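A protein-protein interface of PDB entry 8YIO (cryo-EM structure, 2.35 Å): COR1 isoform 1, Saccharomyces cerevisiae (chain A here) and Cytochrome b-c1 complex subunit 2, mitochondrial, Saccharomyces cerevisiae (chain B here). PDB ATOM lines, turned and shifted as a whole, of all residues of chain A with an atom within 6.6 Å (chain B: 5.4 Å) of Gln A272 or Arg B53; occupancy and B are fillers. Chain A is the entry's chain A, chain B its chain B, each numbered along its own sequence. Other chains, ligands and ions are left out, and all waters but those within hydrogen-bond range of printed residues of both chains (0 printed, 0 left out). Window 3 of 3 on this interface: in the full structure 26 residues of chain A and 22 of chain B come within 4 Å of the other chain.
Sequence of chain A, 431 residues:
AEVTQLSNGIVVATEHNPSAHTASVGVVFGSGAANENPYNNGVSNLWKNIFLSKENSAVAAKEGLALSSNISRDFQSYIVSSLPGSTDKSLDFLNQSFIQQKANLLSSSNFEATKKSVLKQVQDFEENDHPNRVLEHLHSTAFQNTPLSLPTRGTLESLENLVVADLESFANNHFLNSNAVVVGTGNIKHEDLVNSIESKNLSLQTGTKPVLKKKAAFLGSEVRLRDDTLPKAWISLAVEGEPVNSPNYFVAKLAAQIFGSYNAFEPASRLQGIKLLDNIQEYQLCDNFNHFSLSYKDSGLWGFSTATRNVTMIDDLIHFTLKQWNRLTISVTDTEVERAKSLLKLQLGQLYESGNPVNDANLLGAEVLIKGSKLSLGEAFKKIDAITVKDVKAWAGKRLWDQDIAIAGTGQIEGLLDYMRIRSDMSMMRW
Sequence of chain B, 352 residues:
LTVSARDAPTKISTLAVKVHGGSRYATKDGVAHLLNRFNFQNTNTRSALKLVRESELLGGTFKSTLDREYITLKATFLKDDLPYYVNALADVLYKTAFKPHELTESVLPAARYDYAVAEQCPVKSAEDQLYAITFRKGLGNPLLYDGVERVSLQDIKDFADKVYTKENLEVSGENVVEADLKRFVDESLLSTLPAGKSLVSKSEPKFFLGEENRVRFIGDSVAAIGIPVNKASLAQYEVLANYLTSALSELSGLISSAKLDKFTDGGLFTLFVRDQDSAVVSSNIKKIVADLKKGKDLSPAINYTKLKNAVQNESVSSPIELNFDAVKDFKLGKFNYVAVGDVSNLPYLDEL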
ATOM      1  N   PHE A 259      -7.839  23.817  20.439  1.00  0.00           N
ATOM      2  CA  PHE A 259      -8.426  22.512  20.164  1.00  0.00           C
ATOM      3  C   PHE A 259      -9.951  22.542  20.123  1.00  0.00           C
ATOM      4  O   PHE A 259     -10.548  21.793  19.346  1.00  0.00           O
ATOM      5  CB  PHE A 259      -7.917  21.500  21.190  1.00  0.00           C
ATOM      6  CG  PHE A 259      -6.421  21.436  21.265  1.00  0.00           C
ATOM      7  CD1 PHE A 259      -5.684  20.919  20.210  1.00  0.00           C
ATOM      8  CD2 PHE A 259      -5.746  21.925  22.370  1.00  0.00           C
ATOM      9  CE1 PHE A 259      -4.304  20.874  20.262  1.00  0.00           C
ATOM     10  CE2 PHE A 259      -4.366  21.882  22.430  1.00  0.00           C
ATOM     11  CZ  PHE A 259      -3.646  21.356  21.375  1.00  0.00           C
ATOM     12  N   GLY A 260     -10.592  23.384  20.933  1.00  0.00           N
ATOM     13  CA  GLY A 260     -11.987  23.755  20.741  1.00  0.00           C
ATOM     14  C   GLY A 260     -13.019  22.668  21.014  1.00  0.00           C
ATOM     15  O   GLY A 260     -12.831  21.776  21.842  1.00  0.00           O
ATOM     16  N   SER A 261     -14.141  22.768  20.298  1.00  0.00           N
ATOM     17  CA  SER A 261     -15.290  21.886  20.457  1.00  0.00           C
ATOM     18  C   SER A 261     -15.665  21.285  19.109  1.00  0.00           C
ATOM     19  O   SER A 261     -15.288  21.796  18.055  1.00  0.00           O
ATOM     20  CB  SER A 261     -16.498  22.628  21.041  1.00  0.00           C
ATOM     21  OG  SER A 261     -16.223  23.123  22.332  1.00  0.00           O
ATOM     22  N   TYR A 262     -16.429  20.195  19.150  1.00  0.00           N
ATOM     23  CA  TYR A 262     -16.733  19.434  17.945  1.00  0.00           C
ATOM     24  C   TYR A 262     -18.071  18.721  18.097  1.00  0.00           C
ATOM     25  O   TYR A 262     -18.433  18.277  19.185  1.00  0.00           O
ATOM     26  CB  TYR A 262     -15.604  18.437  17.655  1.00  0.00           C
ATOM     27  CG  TYR A 262     -15.867  17.427  16.563  1.00  0.00           C
ATOM     28  CD1 TYR A 262     -16.110  17.827  15.255  1.00  0.00           C
ATOM     29  CD2 TYR A 262     -15.848  16.066  16.841  1.00  0.00           C
ATOM     30  CE1 TYR A 262     -16.339  16.900  14.260  1.00  0.00           C
ATOM     31  CE2 TYR A 262     -16.073  15.135  15.857  1.00  0.00           C
ATOM     32  CZ  TYR A 262     -16.315  15.555  14.570  1.00  0.00           C
ATOM     33  OH  TYR A 262     -16.538  14.620  13.595  1.00  0.00           O
ATOM     34  N   ASN A 263     -18.805  18.633  16.989  1.00  0.00           N
ATOM     35  CA  ASN A 263     -20.050  17.876  16.895  1.00  0.00           C
ATOM     36  C   ASN A 263     -20.038  17.153  15.556  1.00  0.00           C
ATOM     37  O   ASN A 263     -20.038  17.798  14.505  1.00  0.00           O
ATOM     38  CB  ASN A 263     -21.271  18.800  17.018  1.00  0.00           C
ATOM     39  CG  ASN A 263     -22.592  18.048  17.218  1.00  0.00           C
ATOM     40  OD1 ASN A 263     -22.703  16.849  16.970  1.00  0.00           O
ATOM     41  ND2 ASN A 263     -23.605  18.771  17.660  1.00  0.00           N
ATOM     42  N   PRO A 267     -22.742  19.735  10.060  1.00  0.00           N
ATOM     43  CA  PRO A 267     -21.810  19.766   8.917  1.00  0.00           C
ATOM     44  C   PRO A 267     -20.770  20.875   8.970  1.00  0.00           C
ATOM     45  O   PRO A 267     -19.648  20.663   8.499  1.00  0.00           O
ATOM     46  CB  PRO A 267     -22.747  19.932   7.713  1.00  0.00           C
ATOM     47  CG  PRO A 267     -24.064  19.423   8.186  1.00  0.00           C
ATOM     48  CD  PRO A 267     -24.146  19.800   9.626  1.00  0.00           C
ATOM     49  N   ALA A 268     -21.092  22.042   9.526  1.00  0.00           N
ATOM     50  CA  ALA A 268     -20.097  23.105   9.625  1.00  0.00           C
ATOM     51  C   ALA A 268     -19.089  22.867  10.739  1.00  0.00           C
ATOM     52  O   ALA A 268     -17.992  23.432  10.691  1.00  0.00           O
ATOM     53  CB  ALA A 268     -20.779  24.457   9.832  1.00  0.00           C
ATOM     54  N   SER A 269     -19.431  22.045  11.733  1.00  0.00           N
ATOM     55  CA  SER A 269     -18.488  21.708  12.793  1.00  0.00           C
ATOM     56  C   SER A 269     -17.375  20.799  12.283  1.00  0.00           C
ATOM     57  O   SER A 269     -16.283  20.776  12.855  1.00  0.00           O
ATOM     58  CB  SER A 269     -19.239  21.055  13.956  1.00  0.00           C
ATOM     59  OG  SER A 269     -18.370  20.679  15.003  1.00  0.00           O
ATOM     60  N   ARG A 270     -17.629  20.062  11.206  1.00  0.00           N
ATOM     61  CA  ARG A 270     -16.654  19.161  10.607  1.00  0.00           C
ATOM     62  C   ARG A 270     -15.599  19.874   9.767  1.00  0.00           C
ATOM     63  O   ARG A 270     -14.603  19.245   9.399  1.00  0.00           O
ATOM     64  CB  ARG A 270     -17.383  18.123   9.751  1.00  0.00           C
ATOM     65  CG  ARG A 270     -18.345  17.254  10.542  1.00  0.00           C
ATOM     66  CD  ARG A 270     -19.128  16.313   9.646  1.00  0.00           C
ATOM     67  NE  ARG A 270     -18.265  15.341   8.991  1.00  0.00           N
ATOM     68  CZ  ARG A 270     -17.936  14.161   9.504  1.00  0.00           C
ATOM     69  NH1 ARG A 270     -17.138  13.345   8.832  1.00  0.00           N
ATOM     70  NH2 ARG A 270     -18.403  13.793  10.688  1.00  0.00           N
ATOM     71  N   LEU A 271     -15.775  21.161   9.468  1.00  0.00           N
ATOM     72  CA  LEU A 271     -14.878  21.896   8.586  1.00  0.00           C
ATOM     73  C   LEU A 271     -13.982  22.889   9.328  1.00  0.00           C
ATOM     74  O   LEU A 271     -13.404  23.775   8.698  1.00  0.00           O
ATOM     75  CB  LEU A 271     -15.681  22.626   7.507  1.00  0.00           C
ATOM     76  CG  LEU A 271     -16.677  21.836   6.652  1.00  0.00           C
ATOM     77  CD1 LEU A 271     -17.485  22.771   5.768  1.00  0.00           C
ATOM     78  CD2 LEU A 271     -15.977  20.782   5.813  1.00  0.00           C
ATOM     79  N   GLN A 272     -13.845  22.759  10.646  1.00  0.00           N
ATOM     80  CA  GLN A 272     -13.073  23.717  11.429  1.00  0.00           C
ATOM     81  C   GLN A 272     -11.574  23.523  11.231  1.00  0.00           C
ATOM     82  O   GLN A 272     -11.100  22.428  10.921  1.00  0.00           O
ATOM     83  CB  GLN A 272     -13.389  23.641  12.922  1.00  0.00           C
ATOM     84  CG  GLN A 272     -14.789  24.047  13.304  1.00  0.00           C
ATOM     85  CD  GLN A 272     -15.083  23.775  14.764  1.00  0.00           C
ATOM     86  OE1 GLN A 272     -15.036  24.673  15.599  1.00  0.00           O
ATOM     87  NE2 GLN A 272     -15.380  22.527  15.078  1.00  0.00           N
ATOM     88  N   GLY A 273     -10.821  24.602  11.441  1.00  0.00           N
ATOM     89  CA  GLY A 273      -9.377  24.575  11.303  1.00  0.00           C
ATOM     90  C   GLY A 273      -8.635  23.990  12.489  1.00  0.00           C
ATOM     91  O   GLY A 273      -7.793  24.655  13.093  1.00  0.00           O
ATOM     92  N   ILE A 274      -8.938  22.742  12.828  1.00  0.00           N
ATOM     93  CA  ILE A 274      -8.322  22.028  13.940  1.00  0.00           C
ATOM     94  C   ILE A 274      -7.665  20.780  13.370  1.00  0.00           C
ATOM     95  O   ILE A 274      -8.328  19.978  12.701  1.00  0.00           O
ATOM     96  CB  ILE A 274      -9.353  21.669  15.023  1.00  0.00           C
ATOM     97  CG1 ILE A 274     -10.035  22.931  15.557  1.00  0.00           C
ATOM     98  CG2 ILE A 274      -8.710  20.879  16.150  1.00  0.00           C
ATOM     99  CD1 ILE A 274     -11.383  22.691  16.178  1.00  0.00           C
ATOM    100  N   LYS A 275      -6.366  20.613  13.632  1.00  0.00           N
ATOM    101  CA  LYS A 275      -5.617  19.503  13.051  1.00  0.00           C
ATOM    102  C   LYS A 275      -5.944  18.162  13.699  1.00  0.00           C
ATOM    103  O   LYS A 275      -5.606  17.121  13.129  1.00  0.00           O
ATOM    104  CB  LYS A 275      -4.115  19.764  13.153  1.00  0.00           C
ATOM    105  CG  LYS A 275      -3.627  20.950  12.345  1.00  0.00           C
ATOM    106  CD  LYS A 275      -2.112  20.965  12.256  1.00  0.00           C
ATOM    107  CE  LYS A 275      -1.594  22.295  11.738  1.00  0.00           C
ATOM    108  NZ  LYS A 275      -2.109  22.605  10.379  1.00  0.00           N
ATOM    109  N   LEU A 277      -8.934  16.998  14.004  1.00  0.00           N
ATOM    110  CA  LEU A 277     -10.089  16.455  13.294  1.00  0.00           C
ATOM    111  C   LEU A 277      -9.721  15.562  12.115  1.00  0.00           C
ATOM    112  O   LEU A 277     -10.596  14.856  11.609  1.00  0.00           O
ATOM    113  CB  LEU A 277     -10.991  17.590  12.805  1.00  0.00           C
ATOM    114  CG  LEU A 277     -11.643  18.484  13.861  1.00  0.00           C
ATOM    115  CD1 LEU A 277     -12.538  19.521  13.208  1.00  0.00           C
ATOM    116  CD2 LEU A 277     -12.423  17.658  14.875  1.00  0.00           C
ATOM    117  N   ASP A 278      -8.465  15.567  11.665  1.00  0.00           N
ATOM    118  CA  ASP A 278      -8.057  14.658  10.597  1.00  0.00           C
ATOM    119  C   ASP A 278      -7.996  13.213  11.083  1.00  0.00           C
ATOM    120  O   ASP A 278      -8.399  12.295  10.362  1.00  0.00           O
ATOM    121  CB  ASP A 278      -6.707  15.085  10.029  1.00  0.00           C
ATOM    122  CG  ASP A 278      -6.790  16.359   9.219  1.00  0.00           C
ATOM    123  OD1 ASP A 278      -7.857  16.622   8.630  1.00  0.00           O
ATOM    124  OD2 ASP A 278      -5.786  17.099   9.167  1.00  0.00           O
ATOM    125  N   ARG A 339      -5.834  32.287  14.796  1.00  0.00           N
ATOM    126  CA  ARG A 339      -7.208  31.801  14.737  1.00  0.00           C
ATOM    127  C   ARG A 339      -7.826  31.722  16.128  1.00  0.00           C
ATOM    128  O   ARG A 339      -8.992  32.088  16.317  1.00  0.00           O
ATOM    129  CB  ARG A 339      -7.252  30.434  14.049  1.00  0.00           C
ATOM    130  CG  ARG A 339      -8.630  29.784  14.003  1.00  0.00           C
ATOM    131  CD  ARG A 339      -8.539  28.300  13.687  1.00  0.00           C
ATOM    132  NE  ARG A 339      -9.818  27.615  13.855  1.00  0.00           N
ATOM    133  CZ  ARG A 339     -10.216  27.014  14.974  1.00  0.00           C
ATOM    134  NH1 ARG A 339     -11.398  26.418  15.022  1.00  0.00           N
ATOM    135  NH2 ARG A 339      -9.439  27.012  16.046  1.00  0.00           N
ATOM    136  N   LEU A 343     -11.343  33.732  17.907  1.00  0.00           N
ATOM    137  CA  LEU A 343     -12.437  32.942  18.457  1.00  0.00           C
ATOM    138  C   LEU A 343     -12.582  33.123  19.964  1.00  0.00           C
ATOM    139  O   LEU A 343     -13.699  33.035  20.481  1.00  0.00           O
ATOM    140  CB  LEU A 343     -12.249  31.469  18.103  1.00  0.00           C
ATOM    141  CG  LEU A 343     -12.412  31.144  16.614  1.00  0.00           C
ATOM    142  CD1 LEU A 343     -12.193  29.675  16.353  1.00  0.00           C
ATOM    143  CD2 LEU A 343     -13.769  31.580  16.088  1.00  0.00           C
ATOM    144  N   LEU B  49     -16.014  24.891   2.709  1.00  0.00           N
ATOM    145  CA  LEU B  49     -14.800  24.825   3.517  1.00  0.00           C
ATOM    146  C   LEU B  49     -14.088  26.171   3.562  1.00  0.00           C
ATOM    147  O   LEU B  49     -13.568  26.569   4.609  1.00  0.00           O
ATOM    148  CB  LEU B  49     -13.871  23.740   2.970  1.00  0.00           C
ATOM    149  CG  LEU B  49     -12.454  23.639   3.540  1.00  0.00           C
ATOM    150  CD1 LEU B  49     -12.475  23.084   4.951  1.00  0.00           C
ATOM    151  CD2 LEU B  49     -11.577  22.788   2.646  1.00  0.00           C
ATOM    152  N   LYS B  50     -14.068  26.889   2.436  1.00  0.00           N
ATOM    153  CA  LYS B  50     -13.427  28.199   2.373  1.00  0.00           C
ATOM    154  C   LYS B  50     -14.165  29.235   3.216  1.00  0.00           C
ATOM    155  O   LYS B  50     -13.527  30.103   3.820  1.00  0.00           O
ATOM    156  CB  LYS B  50     -13.333  28.645   0.910  1.00  0.00           C
ATOM    157  CG  LYS B  50     -12.675  29.990   0.663  1.00  0.00           C
ATOM    158  CD  LYS B  50     -11.243  30.017   1.153  1.00  0.00           C
ATOM    159  CE  LYS B  50     -10.535  31.281   0.695  1.00  0.00           C
ATOM    160  NZ  LYS B  50      -9.243  31.495   1.401  1.00  0.00           N
ATOM    161  N   LEU B  51     -15.496  29.144   3.290  1.00  0.00           N
ATOM    162  CA  LEU B  51     -16.279  30.084   4.088  1.00  0.00           C
ATOM    163  C   LEU B  51     -16.039  29.910   5.586  1.00  0.00           C
ATOM    164  O   LEU B  51     -16.040  30.898   6.326  1.00  0.00           O
ATOM    165  CB  LEU B  51     -17.765  29.925   3.762  1.00  0.00           C
ATOM    166  CG  LEU B  51     -18.757  30.897   4.410  1.00  0.00           C
ATOM    167  CD1 LEU B  51     -18.703  32.261   3.747  1.00  0.00           C
ATOM    168  CD2 LEU B  51     -20.166  30.340   4.383  1.00  0.00           C
ATOM    169  N   VAL B  52     -15.816  28.677   6.047  1.00  0.00           N
ATOM    170  CA  VAL B  52     -15.587  28.437   7.469  1.00  0.00           C
ATOM    171  C   VAL B  52     -14.194  28.909   7.877  1.00  0.00           C
ATOM    172  O   VAL B  52     -14.026  29.556   8.918  1.00  0.00           O
ATOM    173  CB  VAL B  52     -15.818  26.947   7.799  1.00  0.00           C
ATOM    174  CG1 VAL B  52     -15.261  26.573   9.169  1.00  0.00           C
ATOM    175  CG2 VAL B  52     -17.294  26.617   7.735  1.00  0.00           C
ATOM    176  N   ARG B  53     -13.181  28.626   7.050  1.00  0.00           N
ATOM    177  CA  ARG B  53     -11.808  29.002   7.375  1.00  0.00           C
ATOM    178  C   ARG B  53     -11.592  30.511   7.336  1.00  0.00           C
ATOM    179  O   ARG B  53     -10.798  31.036   8.122  1.00  0.00           O
ATOM    180  CB  ARG B  53     -10.829  28.321   6.418  1.00  0.00           C
ATOM    181  CG  ARG B  53     -10.833  26.809   6.465  1.00  0.00           C
ATOM    182  CD  ARG B  53     -10.473  26.278   7.833  1.00  0.00           C
ATOM    183  NE  ARG B  53     -10.539  24.822   7.876  1.00  0.00           N
ATOM    184  CZ  ARG B  53      -9.514  24.019   7.617  1.00  0.00           C
ATOM    185  NH1 ARG B  53      -9.667  22.708   7.677  1.00  0.00           N
ATOM    186  NH2 ARG B  53      -8.335  24.526   7.296  1.00  0.00           N
ATOM    187  N   GLU B  54     -12.286  31.221   6.447  1.00  0.00           N
ATOM    188  CA  GLU B  54     -12.086  32.662   6.328  1.00  0.00           C
ATOM    189  C   GLU B  54     -12.748  33.428   7.467  1.00  0.00           C
ATOM    190  O   GLU B  54     -12.165  34.378   7.997  1.00  0.00           O
ATOM    191  CB  GLU B  54     -12.624  33.164   4.989  1.00  0.00           C
ATOM    192  CG  GLU B  54     -11.627  33.110   3.857  1.00  0.00           C
ATOM    193  CD  GLU B  54     -12.097  33.867   2.631  1.00  0.00           C
ATOM    194  OE1 GLU B  54     -13.321  33.939   2.402  1.00  0.00           O
ATOM    195  OE2 GLU B  54     -11.240  34.390   1.891  1.00  0.00           O
ATOM    196  N   SER B  55     -13.964  33.039   7.850  1.00  0.00           N
ATOM    197  CA  SER B  55     -14.680  33.764   8.889  1.00  0.00           C
ATOM    198  C   SER B  55     -14.188  33.424  10.289  1.00  0.00           C
ATOM    199  O   SER B  55     -14.435  34.201  11.214  1.00  0.00           O
ATOM    200  CB  SER B  55     -16.183  33.497   8.777  1.00  0.00           C
ATOM    201  OG  SER B  55     -16.473  32.118   8.877  1.00  0.00           O
ATOM    202  N   GLU B  56     -13.498  32.293  10.461  1.00  0.00           N
ATOM    203  CA  GLU B  56     -12.897  31.975  11.752  1.00  0.00           C
ATOM    204  C   GLU B  56     -11.732  32.902  12.066  1.00  0.00           C
ATOM    205  O   GLU B  56     -11.512  33.250  13.231  1.00  0.00           O
ATOM    206  CB  GLU B  56     -12.423  30.523  11.772  1.00  0.00           C
ATOM    207  CG  GLU B  56     -13.456  29.521  12.223  1.00  0.00           C
ATOM    208  CD  GLU B  56     -12.951  28.093  12.135  1.00  0.00           C
ATOM    209  OE1 GLU B  56     -11.934  27.858  11.453  1.00  0.00           O
ATOM    210  OE2 GLU B  56     -13.572  27.204  12.747  1.00  0.00           O
ATOM    211  N   LEU B  57     -10.972  33.301  11.046  1.00  0.00           N
ATOM    212  CA  LEU B  57      -9.855  34.214  11.242  1.00  0.00           C
ATOM    213  C   LEU B  57     -10.308  35.650  11.458  1.00  0.00           C
ATOM    214  O   LEU B  57      -9.541  36.451  12.000  1.00  0.00           O
ATOM    215  CB  LEU B  57      -8.897  34.134  10.052  1.00  0.00           C
ATOM    216  CG  LEU B  57      -8.029  32.872  10.019  1.00  0.00           C
ATOM    217  CD1 LEU B  57      -7.522  32.591   8.618  1.00  0.00           C
ATOM    218  CD2 LEU B  57      -6.871  32.986  10.993  1.00  0.00           C
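The backbone carbonyl oxygen (O) of Leu A271 lies within hydrogen-bond range of the guanidinium group (NE) of Arg B53 (3.2 Å).
The guanidinium group of Arg A339 lies within salt-bridge range of the side-chain carboxylate of Glu B56.
N of Gly A273 lies within hydrogen-bond range of OE1 of Glu B56.
O of Ser A269 is in hydrogen-bond range of NE2 of Gln A272, 3.0 Å away.
O of Ser A261 is in hydrogen-bond range of NE2 of Gln A272 (3.1 Å).
Printed residues of chain B that touch a printed residue of chain A: Leu B49, Val B52, Arg B53, Glu B56 and Leu B57.
Among the printed residues, 9 pairs touch across the chains.
O of Leu A271 touches CD1 of Leu B49 (3.9 Å).
Leu A271 touches Val B52.
Arg B53 touches Gln A272.
Gln A272 touches Glu B56 (CG to OE2, 3.4 Å).
NE of Arg B53 touches N of Gly A273 (3.6 Å).
CA of Arg A339 touches CD2 of Leu B57 (3.9 Å).
Printed residues of chain B within 4 Å of Gln A272: Arg B53 (3.6 Å) and Glu B56 (3.4 Å).
Arg B53 touches just these residues of chain A: Leu A271, Gln A272 and Gly A273.
Printed residues of chain A within 4 Å of Leu B57: Arg A339 (3.9 Å).
Printed residues of chain B within 4 Å of Arg A339: Glu B56 (3.2 Å) and Leu B57 (3.9 Å).
Of the printed residues of chain A, Leu B49 touches Leu A271.
Of the printed residues of chain B, Leu A271 touches Leu B49, Val B52 and Arg B53.
Of the printed residues of chain B, Gly A273 touches Arg B53 and Glu B56.
Leu A343 touches none of the printed residues of chain B.
The nearest residue of chain B that does not touch Gln A272 is Val B52 (4.2 Å).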
